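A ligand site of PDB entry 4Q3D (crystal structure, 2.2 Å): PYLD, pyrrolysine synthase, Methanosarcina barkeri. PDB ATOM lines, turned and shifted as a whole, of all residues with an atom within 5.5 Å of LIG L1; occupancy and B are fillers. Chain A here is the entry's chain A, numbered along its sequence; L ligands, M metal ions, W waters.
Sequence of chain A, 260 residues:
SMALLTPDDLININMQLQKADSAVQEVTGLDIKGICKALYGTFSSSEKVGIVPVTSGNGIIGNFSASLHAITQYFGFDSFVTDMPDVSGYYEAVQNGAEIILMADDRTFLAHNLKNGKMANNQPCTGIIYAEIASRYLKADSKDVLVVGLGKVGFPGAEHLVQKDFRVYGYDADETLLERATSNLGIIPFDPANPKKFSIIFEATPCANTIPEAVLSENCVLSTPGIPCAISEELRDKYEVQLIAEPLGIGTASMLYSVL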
ATOM      1  N   ALA A   3       9.698   7.424  20.148  1.00  0.00           N
ATOM      2  CA  ALA A   3      10.632   7.375  21.332  1.00  0.00           C
ATOM      3  C   ALA A   3      10.355   8.543  22.283  1.00  0.00           C
ATOM      4  O   ALA A   3       9.200   8.928  22.467  1.00  0.00           O
ATOM      5  CB  ALA A   3      12.081   7.339  20.876  1.00  0.00           C
ATOM      6  N   ASN A 122      -1.455  13.504  28.771  1.00  0.00           N
ATOM      7  CA  ASN A 122      -0.928  14.223  27.614  1.00  0.00           C
ATOM      8  C   ASN A 122      -1.270  13.606  26.257  1.00  0.00           C
ATOM      9  O   ASN A 122      -1.386  14.322  25.262  1.00  0.00           O
ATOM     10  CB  ASN A 122       0.598  14.308  27.749  1.00  0.00           C
ATOM     11  CG  ASN A 122       1.260  14.873  26.521  1.00  0.00           C
ATOM     12  OD1 ASN A 122       1.880  14.133  25.764  1.00  0.00           O
ATOM     13  ND2 ASN A 122       1.130  16.182  26.307  1.00  0.00           N
ATOM     14  N   GLN A 123      -1.441  12.274  26.212  1.00  0.00           N
ATOM     15  CA  GLN A 123      -1.680  11.593  24.937  1.00  0.00           C
ATOM     16  C   GLN A 123      -3.036  11.916  24.325  1.00  0.00           C
ATOM     17  O   GLN A 123      -3.109  12.374  23.174  1.00  0.00           O
ATOM     18  CB  GLN A 123      -1.483  10.088  25.061  1.00  0.00           C
ATOM     19  CG  GLN A 123      -0.025   9.656  24.998  1.00  0.00           C
ATOM     20  CD  GLN A 123       0.261   8.427  25.836  1.00  0.00           C
ATOM     21  OE1 GLN A 123      -0.537   8.052  26.696  1.00  0.00           O
ATOM     22  NE2 GLN A 123       1.390   7.800  25.596  1.00  0.00           N
ATOM     23  N   THR A 126      -3.323  15.775  23.592  1.00  0.00           N
ATOM     24  CA  THR A 126      -2.619  16.164  22.363  1.00  0.00           C
ATOM     25  C   THR A 126      -3.399  15.764  21.108  1.00  0.00           C
ATOM     26  O   THR A 126      -3.561  16.574  20.210  1.00  0.00           O
ATOM     27  CB  THR A 126      -1.201  15.560  22.288  1.00  0.00           C
ATOM     28  OG1 THR A 126      -0.413  16.039  23.373  1.00  0.00           O
ATOM     29  CG2 THR A 126      -0.507  15.946  20.979  1.00  0.00           C
ATOM     30  N   TYR A 130      -4.829  18.855  18.494  1.00  0.00           N
ATOM     31  CA  TYR A 130      -4.327  18.827  17.117  1.00  0.00           C
ATOM     32  C   TYR A 130      -5.420  18.426  16.118  1.00  0.00           C
ATOM     33  O   TYR A 130      -5.471  18.975  15.019  1.00  0.00           O
ATOM     34  CB  TYR A 130      -3.115  17.900  16.971  1.00  0.00           C
ATOM     35  CG  TYR A 130      -1.788  18.548  17.325  1.00  0.00           C
ATOM     36  CD1 TYR A 130      -1.032  19.219  16.365  1.00  0.00           C
ATOM     37  CD2 TYR A 130      -1.298  18.493  18.610  1.00  0.00           C
ATOM     38  CE1 TYR A 130       0.179  19.803  16.700  1.00  0.00           C
ATOM     39  CE2 TYR A 130      -0.089  19.068  18.950  1.00  0.00           C
ATOM     40  CZ  TYR A 130       0.652  19.731  17.990  1.00  0.00           C
ATOM     41  OH  TYR A 130       1.856  20.315  18.340  1.00  0.00           O
ATOM     42  N   VAL A 148      -3.764   9.690  10.141  1.00  0.00           N
ATOM     43  CA  VAL A 148      -2.682   8.740   9.923  1.00  0.00           C
ATOM     44  C   VAL A 148      -1.981   8.481  11.261  1.00  0.00           C
ATOM     45  O   VAL A 148      -1.342   9.369  11.817  1.00  0.00           O
ATOM     46  CB  VAL A 148      -1.712   9.272   8.857  1.00  0.00           C
ATOM     47  CG1 VAL A 148      -0.459   8.424   8.772  1.00  0.00           C
ATOM     48  CG2 VAL A 148      -2.408   9.334   7.510  1.00  0.00           C
ATOM     49  N   GLY A 149      -2.113   7.257  11.772  1.00  0.00           N
ATOM     50  CA  GLY A 149      -1.629   6.904  13.095  1.00  0.00           C
ATOM     51  C   GLY A 149      -2.810   6.877  14.033  1.00  0.00           C
ATOM     52  O   GLY A 149      -3.449   7.913  14.268  1.00  0.00           O
ATOM     53  N   LEU A 150      -3.117   5.699  14.569  1.00  0.00           N
ATOM     54  CA  LEU A 150      -4.291   5.493  15.415  1.00  0.00           C
ATOM     55  C   LEU A 150      -3.903   4.860  16.762  1.00  0.00           C
ATOM     56  O   LEU A 150      -4.587   3.978  17.266  1.00  0.00           O
ATOM     57  CB  LEU A 150      -5.328   4.650  14.674  1.00  0.00           C
ATOM     58  CG  LEU A 150      -5.900   5.291  13.401  1.00  0.00           C
ATOM     59  CD1 LEU A 150      -6.617   4.283  12.527  1.00  0.00           C
ATOM     60  CD2 LEU A 150      -6.830   6.440  13.759  1.00  0.00           C
ATOM     61  N   GLY A 151      -2.801   5.329  17.336  1.00  0.00           N
ATOM     62  CA  GLY A 151      -2.344   4.866  18.633  1.00  0.00           C
ATOM     63  C   GLY A 151      -2.841   5.775  19.745  1.00  0.00           C
ATOM     64  O   GLY A 151      -3.948   6.290  19.687  1.00  0.00           O
ATOM     65  N   LYS A 152      -1.998   5.982  20.750  1.00  0.00           N
ATOM     66  CA  LYS A 152      -2.414   6.681  21.959  1.00  0.00           C
ATOM     67  C   LYS A 152      -2.744   8.159  21.754  1.00  0.00           C
ATOM     68  O   LYS A 152      -3.566   8.714  22.462  1.00  0.00           O
ATOM     69  CB  LYS A 152      -1.356   6.489  23.046  1.00  0.00           C
ATOM     70  CG  LYS A 152      -1.263   5.028  23.496  1.00  0.00           C
ATOM     71  CD  LYS A 152      -0.192   4.790  24.539  1.00  0.00           C
ATOM     72  CE  LYS A 152       1.214   4.951  23.987  1.00  0.00           C
ATOM     73  NZ  LYS A 152       1.548   3.966  22.909  1.00  0.00           N
ATOM     74  N   VAL A 153      -2.120   8.785  20.761  1.00  0.00           N
ATOM     75  CA  VAL A 153      -2.447  10.164  20.396  1.00  0.00           C
ATOM     76  C   VAL A 153      -3.521  10.152  19.315  1.00  0.00           C
ATOM     77  O   VAL A 153      -4.503  10.880  19.403  1.00  0.00           O
ATOM     78  CB  VAL A 153      -1.200  10.933  19.907  1.00  0.00           C
ATOM     79  CG1 VAL A 153      -1.576  12.293  19.329  1.00  0.00           C
ATOM     80  CG2 VAL A 153      -0.206  11.106  21.041  1.00  0.00           C
ATOM     81  N   GLY A 154      -3.321   9.305  18.305  1.00  0.00           N
ATOM     82  CA  GLY A 154      -4.177   9.305  17.121  1.00  0.00           C
ATOM     83  C   GLY A 154      -5.609   8.852  17.348  1.00  0.00           C
ATOM     84  O   GLY A 154      -6.541   9.470  16.826  1.00  0.00           O
ATOM     85  N   TYR A 171      -6.012   5.519   8.812  1.00  0.00           N
ATOM     86  CA  TYR A 171      -4.981   4.537   8.451  1.00  0.00           C
ATOM     87  C   TYR A 171      -3.950   4.395   9.561  1.00  0.00           C
ATOM     88  O   TYR A 171      -3.559   5.353  10.217  1.00  0.00           O
ATOM     89  CB  TYR A 171      -4.272   4.907   7.143  1.00  0.00           C
ATOM     90  CG  TYR A 171      -3.252   3.877   6.689  1.00  0.00           C
ATOM     91  CD1 TYR A 171      -3.653   2.619   6.249  1.00  0.00           C
ATOM     92  CD2 TYR A 171      -1.885   4.143   6.744  1.00  0.00           C
ATOM     93  CE1 TYR A 171      -2.727   1.665   5.864  1.00  0.00           C
ATOM     94  CE2 TYR A 171      -0.942   3.206   6.354  1.00  0.00           C
ATOM     95  CZ  TYR A 171      -1.371   1.965   5.906  1.00  0.00           C
ATOM     96  OH  TYR A 171      -0.448   1.027   5.526  1.00  0.00           O
ATOM     97  N   ASP A 172      -3.528   3.153   9.768  1.00  0.00           N
ATOM     98  CA  ASP A 172      -2.376   2.845  10.584  1.00  0.00           C
ATOM     99  C   ASP A 172      -1.684   1.656   9.934  1.00  0.00           C
ATOM    100  O   ASP A 172      -2.343   0.699   9.523  1.00  0.00           O
ATOM    101  CB  ASP A 172      -2.808   2.514  12.018  1.00  0.00           C
ATOM    102  CG  ASP A 172      -1.655   2.555  12.995  1.00  0.00           C
ATOM    103  OD1 ASP A 172      -0.758   1.692  12.873  1.00  0.00           O
ATOM    104  OD2 ASP A 172      -1.646   3.433  13.871  1.00  0.00           O
ATOM    105  N   ALA A 173      -0.363   1.706   9.854  1.00  0.00           N
ATOM    106  CA  ALA A 173       0.394   0.600   9.263  1.00  0.00           C
ATOM    107  C   ALA A 173       0.192  -0.714  10.030  1.00  0.00           C
ATOM    108  O   ALA A 173       0.414  -1.775   9.483  1.00  0.00           O
ATOM    109  CB  ALA A 173       1.870   0.951   9.181  1.00  0.00           C
ATOM    110  N   ASP A 174      -0.214  -0.618  11.297  1.00  0.00           N
ATOM    111  CA  ASP A 174      -0.581  -1.794  12.098  1.00  0.00           C
ATOM    112  C   ASP A 174      -2.061  -2.123  11.884  1.00  0.00           C
ATOM    113  O   ASP A 174      -2.951  -1.415  12.384  1.00  0.00           O
ATOM    114  CB  ASP A 174      -0.286  -1.552  13.580  1.00  0.00           C
ATOM    115  CG  ASP A 174      -0.468  -2.798  14.437  1.00  0.00           C
ATOM    116  OD1 ASP A 174      -1.365  -3.619  14.135  1.00  0.00           O
ATOM    117  OD2 ASP A 174       0.267  -2.954  15.431  1.00  0.00           O
ATOM    118  N   LEU A 177      -4.440  -2.263  14.920  1.00  0.00           N
ATOM    119  CA  LEU A 177      -4.813  -0.926  15.382  1.00  0.00           C
ATOM    120  C   LEU A 177      -5.854  -0.267  14.471  1.00  0.00           C
ATOM    121  O   LEU A 177      -6.683   0.510  14.952  1.00  0.00           O
ATOM    122  CB  LEU A 177      -3.581   0.001  15.497  1.00  0.00           C
ATOM    123  CG  LEU A 177      -2.792   0.108  16.806  1.00  0.00           C
ATOM    124  CD1 LEU A 177      -3.645   0.701  17.918  1.00  0.00           C
ATOM    125  CD2 LEU A 177      -2.222  -1.229  17.250  1.00  0.00           C
ATOM    126  N   ALA A 204      -0.230  11.342  13.540  1.00  0.00           N
ATOM    127  CA  ALA A 204       0.270  11.080  14.893  1.00  0.00           C
ATOM    128  C   ALA A 204       1.131   9.820  14.889  1.00  0.00           C
ATOM    129  O   ALA A 204       0.725   8.794  15.419  1.00  0.00           O
ATOM    130  CB  ALA A 204      -0.903  10.939  15.852  1.00  0.00           C
ATOM    131  N   THR A 205       2.306   9.915  14.264  1.00  0.00           N
ATOM    132  CA  THR A 205       3.283   8.810  14.245  1.00  0.00           C
ATOM    133  C   THR A 205       4.675   9.307  14.609  1.00  0.00           C
ATOM    134  O   THR A 205       4.956  10.511  14.518  1.00  0.00           O
ATOM    135  CB  THR A 205       3.378   8.095  12.869  1.00  0.00           C
ATOM    136  OG1 THR A 205       4.244   8.812  11.991  1.00  0.00           O
ATOM    137  CG2 THR A 205       2.012   7.943  12.219  1.00  0.00           C
ATOM    138  N   PRO A 206       5.574   8.387  15.024  1.00  0.00           N
ATOM    139  CA  PRO A 206       6.986   8.709  15.251  1.00  0.00           C
ATOM    140  C   PRO A 206       7.851   8.520  14.002  1.00  0.00           C
ATOM    141  O   PRO A 206       9.062   8.336  14.116  1.00  0.00           O
ATOM    142  CB  PRO A 206       7.389   7.703  16.319  1.00  0.00           C
ATOM    143  CG  PRO A 206       6.582   6.492  15.982  1.00  0.00           C
ATOM    144  CD  PRO A 206       5.263   7.024  15.488  1.00  0.00           C
ATOM    145  N   CYS A 207       7.227   8.575  12.822  1.00  0.00           N
ATOM    146  CA  CYS A 207       7.908   8.241  11.570  1.00  0.00           C
ATOM    147  C   CYS A 207       7.844   9.368  10.540  1.00  0.00           C
ATOM    148  O   CYS A 207       6.932  10.191  10.542  1.00  0.00           O
ATOM    149  CB  CYS A 207       7.306   6.975  10.974  1.00  0.00           C
ATOM    150  SG  CYS A 207       7.403   5.535  12.056  1.00  0.00           S
ATOM    151  N   THR A 210       5.116   9.775   6.182  1.00  0.00           N
ATOM    152  CA  THR A 210       3.932   8.930   6.333  1.00  0.00           C
ATOM    153  C   THR A 210       2.726   9.460   5.561  1.00  0.00           C
ATOM    154  O   THR A 210       1.687   8.807   5.512  1.00  0.00           O
ATOM    155  CB  THR A 210       3.559   8.768   7.821  1.00  0.00           C
ATOM    156  OG1 THR A 210       3.349  10.050   8.404  1.00  0.00           O
ATOM    157  CG2 THR A 210       4.660   8.054   8.570  1.00  0.00           C
ATOM    158  N   THR A 224       0.102  17.924  13.035  1.00  0.00           N
ATOM    159  CA  THR A 224       0.860  16.762  13.489  1.00  0.00           C
ATOM    160  C   THR A 224       1.731  17.029  14.721  1.00  0.00           C
ATOM    161  O   THR A 224       2.643  17.863  14.686  1.00  0.00           O
ATOM    162  CB  THR A 224       1.693  16.147  12.336  1.00  0.00           C
ATOM    163  OG1 THR A 224       2.428  15.015  12.824  1.00  0.00           O
ATOM    164  CG2 THR A 224       2.650  17.163  11.712  1.00  0.00           C
ATOM    165  N   PRO A 225       1.426  16.323  15.833  1.00  0.00           N
ATOM    166  CA  PRO A 225       2.300  16.291  17.014  1.00  0.00           C
ATOM    167  C   PRO A 225       3.529  15.421  16.778  1.00  0.00           C
ATOM    168  O   PRO A 225       4.502  15.545  17.503  1.00  0.00           O
ATOM    169  CB  PRO A 225       1.405  15.677  18.086  1.00  0.00           C
ATOM    170  CG  PRO A 225       0.441  14.822  17.340  1.00  0.00           C
ATOM    171  CD  PRO A 225       0.180  15.567  16.067  1.00  0.00           C
ATOM    172  N   GLY A 226       3.474  14.564  15.765  1.00  0.00           N
ATOM    173  CA  GLY A 226       4.521  13.572  15.488  1.00  0.00           C
ATOM    174  C   GLY A 226       5.924  14.107  15.257  1.00  0.00           C
ATOM    175  O   GLY A 226       6.116  15.204  14.735  1.00  0.00           O
ATOM    176  N   ILE A 227       6.915  13.310  15.673  1.00  0.00           N
ATOM    177  CA  ILE A 227       8.318  13.652  15.545  1.00  0.00           C
ATOM    178  C   ILE A 227       9.065  12.398  15.062  1.00  0.00           C
ATOM    179  O   ILE A 227       8.956  11.349  15.691  1.00  0.00           O
ATOM    180  CB  ILE A 227       8.913  14.137  16.897  1.00  0.00           C
ATOM    181  CG1 ILE A 227       7.988  15.161  17.566  1.00  0.00           C
ATOM    182  CG2 ILE A 227      10.303  14.743  16.709  1.00  0.00           C
ATOM    183  CD1 ILE A 227       8.305  15.464  19.018  1.00  0.00           C
ATOM    184  N   GLU A 246       4.657  21.099  16.608  1.00  0.00           N
ATOM    185  CA  GLU A 246       5.322  21.735  17.720  1.00  0.00           C
ATOM    186  C   GLU A 246       5.462  20.637  18.771  1.00  0.00           C
ATOM    187  O   GLU A 246       4.560  19.814  18.919  1.00  0.00           O
ATOM    188  CB  GLU A 246       4.478  22.927  18.160  1.00  0.00           C
ATOM    189  CG  GLU A 246       5.076  23.792  19.245  1.00  0.00           C
ATOM    190  CD  GLU A 246       4.823  23.221  20.631  1.00  0.00           C
ATOM    191  OE1 GLU A 246       5.647  23.507  21.542  1.00  0.00           O
ATOM    192  OE2 GLU A 246       3.835  22.486  20.812  1.00  0.00           O
ATOM    193  N   PRO A 247       6.608  20.570  19.462  1.00  0.00           N
ATOM    194  CA  PRO A 247       6.911  19.317  20.180  1.00  0.00           C
ATOM    195  C   PRO A 247       6.336  19.133  21.581  1.00  0.00           C
ATOM    196  O   PRO A 247       6.365  18.014  22.080  1.00  0.00           O
ATOM    197  CB  PRO A 247       8.443  19.330  20.250  1.00  0.00           C
ATOM    198  CG  PRO A 247       8.809  20.765  20.241  1.00  0.00           C
ATOM    199  CD  PRO A 247       7.770  21.477  19.425  1.00  0.00           C
ATOM    200  N   LEU A 248       5.812  20.178  22.225  1.00  0.00           N
ATOM    201  CA  LEU A 248       5.427  20.055  23.636  1.00  0.00           C
ATOM    202  C   LEU A 248       4.289  20.963  24.078  1.00  0.00           C
ATOM    203  O   LEU A 248       3.393  20.518  24.813  1.00  0.00           O
ATOM    204  CB  LEU A 248       6.645  20.349  24.519  1.00  0.00           C
ATOM    205  CG  LEU A 248       6.533  20.088  26.016  1.00  0.00           C
ATOM    206  CD1 LEU A 248       6.105  18.659  26.314  1.00  0.00           C
ATOM    207  CD2 LEU A 248       7.873  20.374  26.668  1.00  0.00           C
ATOM    208  N   GLY A 249       4.334  22.223  23.653  1.00  0.00           N
ATOM    209  CA  GLY A 249       3.477  23.275  24.175  1.00  0.00           C
ATOM    210  C   GLY A 249       1.983  23.250  23.868  1.00  0.00           C
ATOM    211  O   GLY A 249       1.182  23.609  24.720  1.00  0.00           O
ATOM    212  N   GLY A 251       0.068  20.524  23.074  1.00  0.00           N
ATOM    213  CA  GLY A 251      -0.395  19.427  23.930  1.00  0.00           C
ATOM    214  C   GLY A 251      -0.422  19.785  25.400  1.00  0.00           C
ATOM    215  O   GLY A 251      -1.347  19.385  26.113  1.00  0.00           O
HETATM  216  P1  LIG L   1       1.892   5.218  19.353  1.00  0.00           P
HETATM  217  O1  LIG L   1       3.070   4.294  19.198  1.00  0.00           O
HETATM  218  O2  LIG L   1       0.881   4.986  20.453  1.00  0.00           O
HETATM  219  O3  LIG L   1       1.123   5.250  17.947  1.00  0.00           O
HETATM  220  C1  LIG L   1       1.805   5.628  16.748  1.00  0.00           C
HETATM  221  C2  LIG L   1       1.156   4.876  15.603  1.00  0.00           C
HETATM  222  O4  LIG L   1       1.697   5.277  14.337  1.00  0.00           O
HETATM  223  C3  LIG L   1       1.373   3.371  15.718  1.00  0.00           C
HETATM  224  O5  LIG L   1       0.107   2.716  15.908  1.00  0.00           O
HETATM  225  C4  LIG L   1       2.015   2.965  14.400  1.00  0.00           C
HETATM  226  O6  LIG L   1       1.534   1.741  13.846  1.00  0.00           O
HETATM  227  C5  LIG L   1       1.657   4.123  13.501  1.00  0.00           C
HETATM  228  N1  LIG L   1       2.534   4.218  12.305  1.00  0.00           N
HETATM  229  C6  LIG L   1       3.872   4.088  12.227  1.00  0.00           C
HETATM  230  N2  LIG L   1       4.290   4.240  10.945  1.00  0.00           N
HETATM  231  C7  LIG L   1       3.209   4.459  10.178  1.00  0.00           C
HETATM  232  C8  LIG L   1       2.910   4.705   8.746  1.00  0.00           C
HETATM  233  N3  LIG L   1       3.905   4.734   7.837  1.00  0.00           N
HETATM  234  N4  LIG L   1       1.627   4.889   8.383  1.00  0.00           N
HETATM  235  C9  LIG L   1       0.618   4.863   9.273  1.00  0.00           C
HETATM  236  N5  LIG L   1       0.809   4.643  10.584  1.00  0.00           N
HETATM  237  C10 LIG L   1       2.050   4.443  11.088  1.00  0.00           C
HETATM  238  O7  LIG L   1       2.473   6.708  19.467  1.00  0.00           O
HETATM  239  P2  LIG L   1       1.666   7.917  20.165  1.00  0.00           P
HETATM  240  O8  LIG L   1       1.931   7.857  21.651  1.00  0.00           O
HETATM  241  O9  LIG L   1       0.255   7.945  19.628  1.00  0.00           O
HETATM  242  O10 LIG L   1       2.464   9.205  19.610  1.00  0.00           O
HETATM  243  C11 LIG L   1       2.807   9.342  18.237  1.00  0.00           C
HETATM  244  C12 LIG L   1       3.818  10.466  18.085  1.00  0.00           C
HETATM  245  O11 LIG L   1       3.333  11.650  18.710  1.00  0.00           O
HETATM  246  C13 LIG L   1       5.166  10.156  18.730  1.00  0.00           C
HETATM  247  O12 LIG L   1       6.225  10.558  17.862  1.00  0.00           O
HETATM  248  C14 LIG L   1       5.197  11.009  19.981  1.00  0.00           C
HETATM  249  O13 LIG L   1       6.523  11.385  20.357  1.00  0.00           O
HETATM  250  C15 LIG L   1       4.385  12.212  19.507  1.00  0.00           C
HETATM  251  N6  LIG L   1       3.814  13.067  20.561  1.00  0.00           N
HETATM  252  C16 LIG L   1       3.952  14.384  20.407  1.00  0.00           C
HETATM  253  C17 LIG L   1       3.428  15.291  21.323  1.00  0.00           C
HETATM  254  C18 LIG L   1       3.593  16.783  21.124  1.00  0.00           C
HETATM  255  O14 LIG L   1       3.323  17.529  22.048  1.00  0.00           O
HETATM  256  N7  LIG L   1       4.025  17.286  19.957  1.00  0.00           N
HETATM  257  C19 LIG L   1       2.743  14.788  22.430  1.00  0.00           C
HETATM  258  C20 LIG L   1       2.603  13.401  22.574  1.00  0.00           C
HETATM  259  C21 LIG L   1       3.144  12.550  21.619  1.00  0.00           C
HETATM  260  O1  LG2 L   2       7.677  12.651  27.270  1.00  0.00           O
HETATM  261  C1  LG2 L   2       7.449  11.742  28.069  1.00  0.00           C
HETATM  262  C2  LG2 L   2       6.239  10.895  27.788  1.00  0.00           C
HETATM  263  N1  LG2 L   2       5.726  10.016  28.899  1.00  0.00           N
HETATM  264  C3  LG2 L   2       6.507  10.057  26.529  1.00  0.00           C
HETATM  265  C4  LG2 L   2       5.317  10.147  25.563  1.00  0.00           C
HETATM  266  C5  LG2 L   2       3.951   9.978  26.249  1.00  0.00           C
HETATM  267  N2  LG2 L   2       3.230  11.271  26.437  1.00  0.00           N
HETATM  268  N3  LG2 L   2       8.278  11.527  29.146  1.00  0.00           N
HETATM  269  C6  LG2 L   2       9.029  12.732  29.539  1.00  0.00           C
HETATM  270  C7  LG2 L   2       9.895  12.427  30.757  1.00  0.00           C
HETATM  271  C8  LG2 L   2      10.260  13.699  31.529  1.00  0.00           C
HETATM  272  C9  LG2 L   2      11.458  13.484  32.446  1.00  0.00           C
HETATM  273  N4  LG2 L   2      11.171  12.429  33.477  1.00  0.00           N
HETATM  274  C10 LG2 L   2      11.816  14.778  33.100  1.00  0.00           C
HETATM  275  O2  LG2 L   2      12.652  15.520  32.607  1.00  0.00           O
HETATM  276  O3  LG2 L   2      11.225  15.145  34.239  1.00  0.00           O
HETATM  277 MG    MG M   1       2.598  19.954  21.348  1.00  0.00          MG
HETATM  278  O   HOH W   1       5.461  12.824  23.748  1.00  0.00           O
HETATM  279  O   HOH W   2       0.192   2.319  20.713  1.00  0.00           O
HETATM  280  O   HOH W   3       2.526  17.874  24.480  1.00  0.00           O
HETATM  281  O   HOH W   4       3.629   0.782  12.123  1.00  0.00           O
HETATM  282  O   HOH W   5       3.094   9.459  23.423  1.00  0.00           O
HETATM  283  O   HOH W   6       5.617   6.383  19.224  1.00  0.00           O
HETATM  284  O   HOH W   7       5.756  15.583  23.462  1.00  0.00           O
HETATM  285  O   HOH W   8       0.961   6.063   5.770  1.00  0.00           O
HETATM  286  O   HOH W   9       1.401  -0.048  16.717  1.00  0.00           O
HETATM  287  O   HOH W  10      -1.249   7.772  17.286  1.00  0.00           O
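OD1 of Asp 172 sits at hydrogen-bond distance from O6 of LIG L1, at 2.5 Å.
N of Lys 152 is in hydrogen-bond range of O2 of LIG L1 (3.1 Å).
NZ of Lys 152 is in salt-bridge range of O2 of LIG L1.
N of Val 153 is in hydrogen-bond range of O9 of LIG L1.
The backbone carbonyl oxygen of Glu 246 lies within hydrogen-bond range of a nitrogen (N7) of LIG L1.
The backbone carbonyl oxygen (O) of Pro 225 is in hydrogen-bond range of a nitrogen (N7) of LIG L1.
N7 of LIG L1 sits close to O of Pro 247 (3.2 Å).
The backbone NH of Ala 173 is in hydrogen-bond range of a nitrogen (N5) of LIG L1, 3.2 Å away.
A nitrogen (N2) of LIG L1 lies within hydrogen-bond range of the side-chain sulfur (SG) of Cys 207 (3.5 Å).
OD1 of Asn 122 lies within hydrogen-bond range of N2 of LG2 L2 (3.2 Å).
OD1 of Asp 172 lies within hydrogen-bond range of N of Asp 174 (2.8 Å).
The backbone NH (N) of Leu 248 lies within hydrogen-bond range of the side-chain carboxylate (OE2) of Glu 246, 3.4 Å away.
OH of Tyr 130 lies within hydrogen-bond range of O of Glu 246, 2.8 Å away.
OE1 of Glu 246 is in hydrogen-bond range of N of Gly 249 (2.8 Å).
The backbone NH of Cys 207 is in hydrogen-bond range of the side-chain hydroxyl of Thr 205 (3.1 Å).
N of Ala 204 sits at hydrogen-bond distance from O of Val 148 (2.8 Å).
N of Gly 149 sits at hydrogen-bond distance from O of Tyr 171 (2.9 Å).
The backbone NH (N) of Leu 177 lies within hydrogen-bond range of the side-chain carboxylate (OD1) of Asp 174, 3.5 Å away.
Merely in contact with LIG L1: Pro 206 (3.3 Å), Asn 122 (3.4 Å), Thr 205 (3.4 Å), Thr 210 (3.5 Å), Thr 126 (3.5 Å), Ala 204 (3.5 Å), Gly 151 (3.6 Å), Ile 227 (3.6 Å), Tyr 171 (3.6 Å), Leu 248 (3.6 Å), Val 148 (3.8 Å), Asp 174 (3.8 Å), Gly 149 (3.9 Å), Gly 226 (3.9 Å) and Gln 123 (3.98 Å).
Hydrophobic or aromatic side chains that line LIG L1: Val 148, Val 153, Tyr 171, Ala 173, Pro 206 and Pro 225.
23 residues have an atom within 4 Å of LIG L1: Asn 122, Gln 123, Thr 126, Val 148, Gly 149, Gly 151, Lys 152, Val 153, Tyr 171, Asp 172, Ala 173, Asp 174, Ala 204, Thr 205, Pro 206, Cys 207, Thr 210, Pro 225, Gly 226, Ile 227, Glu 246, Pro 247 and Leu 248.
The nearest printed residue that does not touch LIG L1 is Leu 177 (4.002 Å).
Water W3 lies within hydrogen-bond range of O14 of LIG L1, O of Leu 248 and ND2 of Asn 122.
Water W5 lies within hydrogen-bond range of O8 of LIG L1 (2.7 Å) and NE2 of Gln 123 (3.2 Å).
Water W2 lies within hydrogen-bond range of O2 of LIG L1 (2.8 Å) and NZ of Lys 152 (3.1 Å).
Water W10 lies within hydrogen-bond range of the backbone NH of Gly 154 (2.8 Å), an oxygen (O9) of LIG L1 (2.8 Å), the backbone NH of Gly 151 (2.9 Å) and the backbone carbonyl oxygen of Ala 204 (2.9 Å).
Water W8 bridges O of Thr 210 (2.9 Å) and N4 of LIG L1 (2.9 Å).
Water W9 bridges O5 of LIG L1 (3.2 Å) and OD2 of Asp 174 (3.4 Å).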
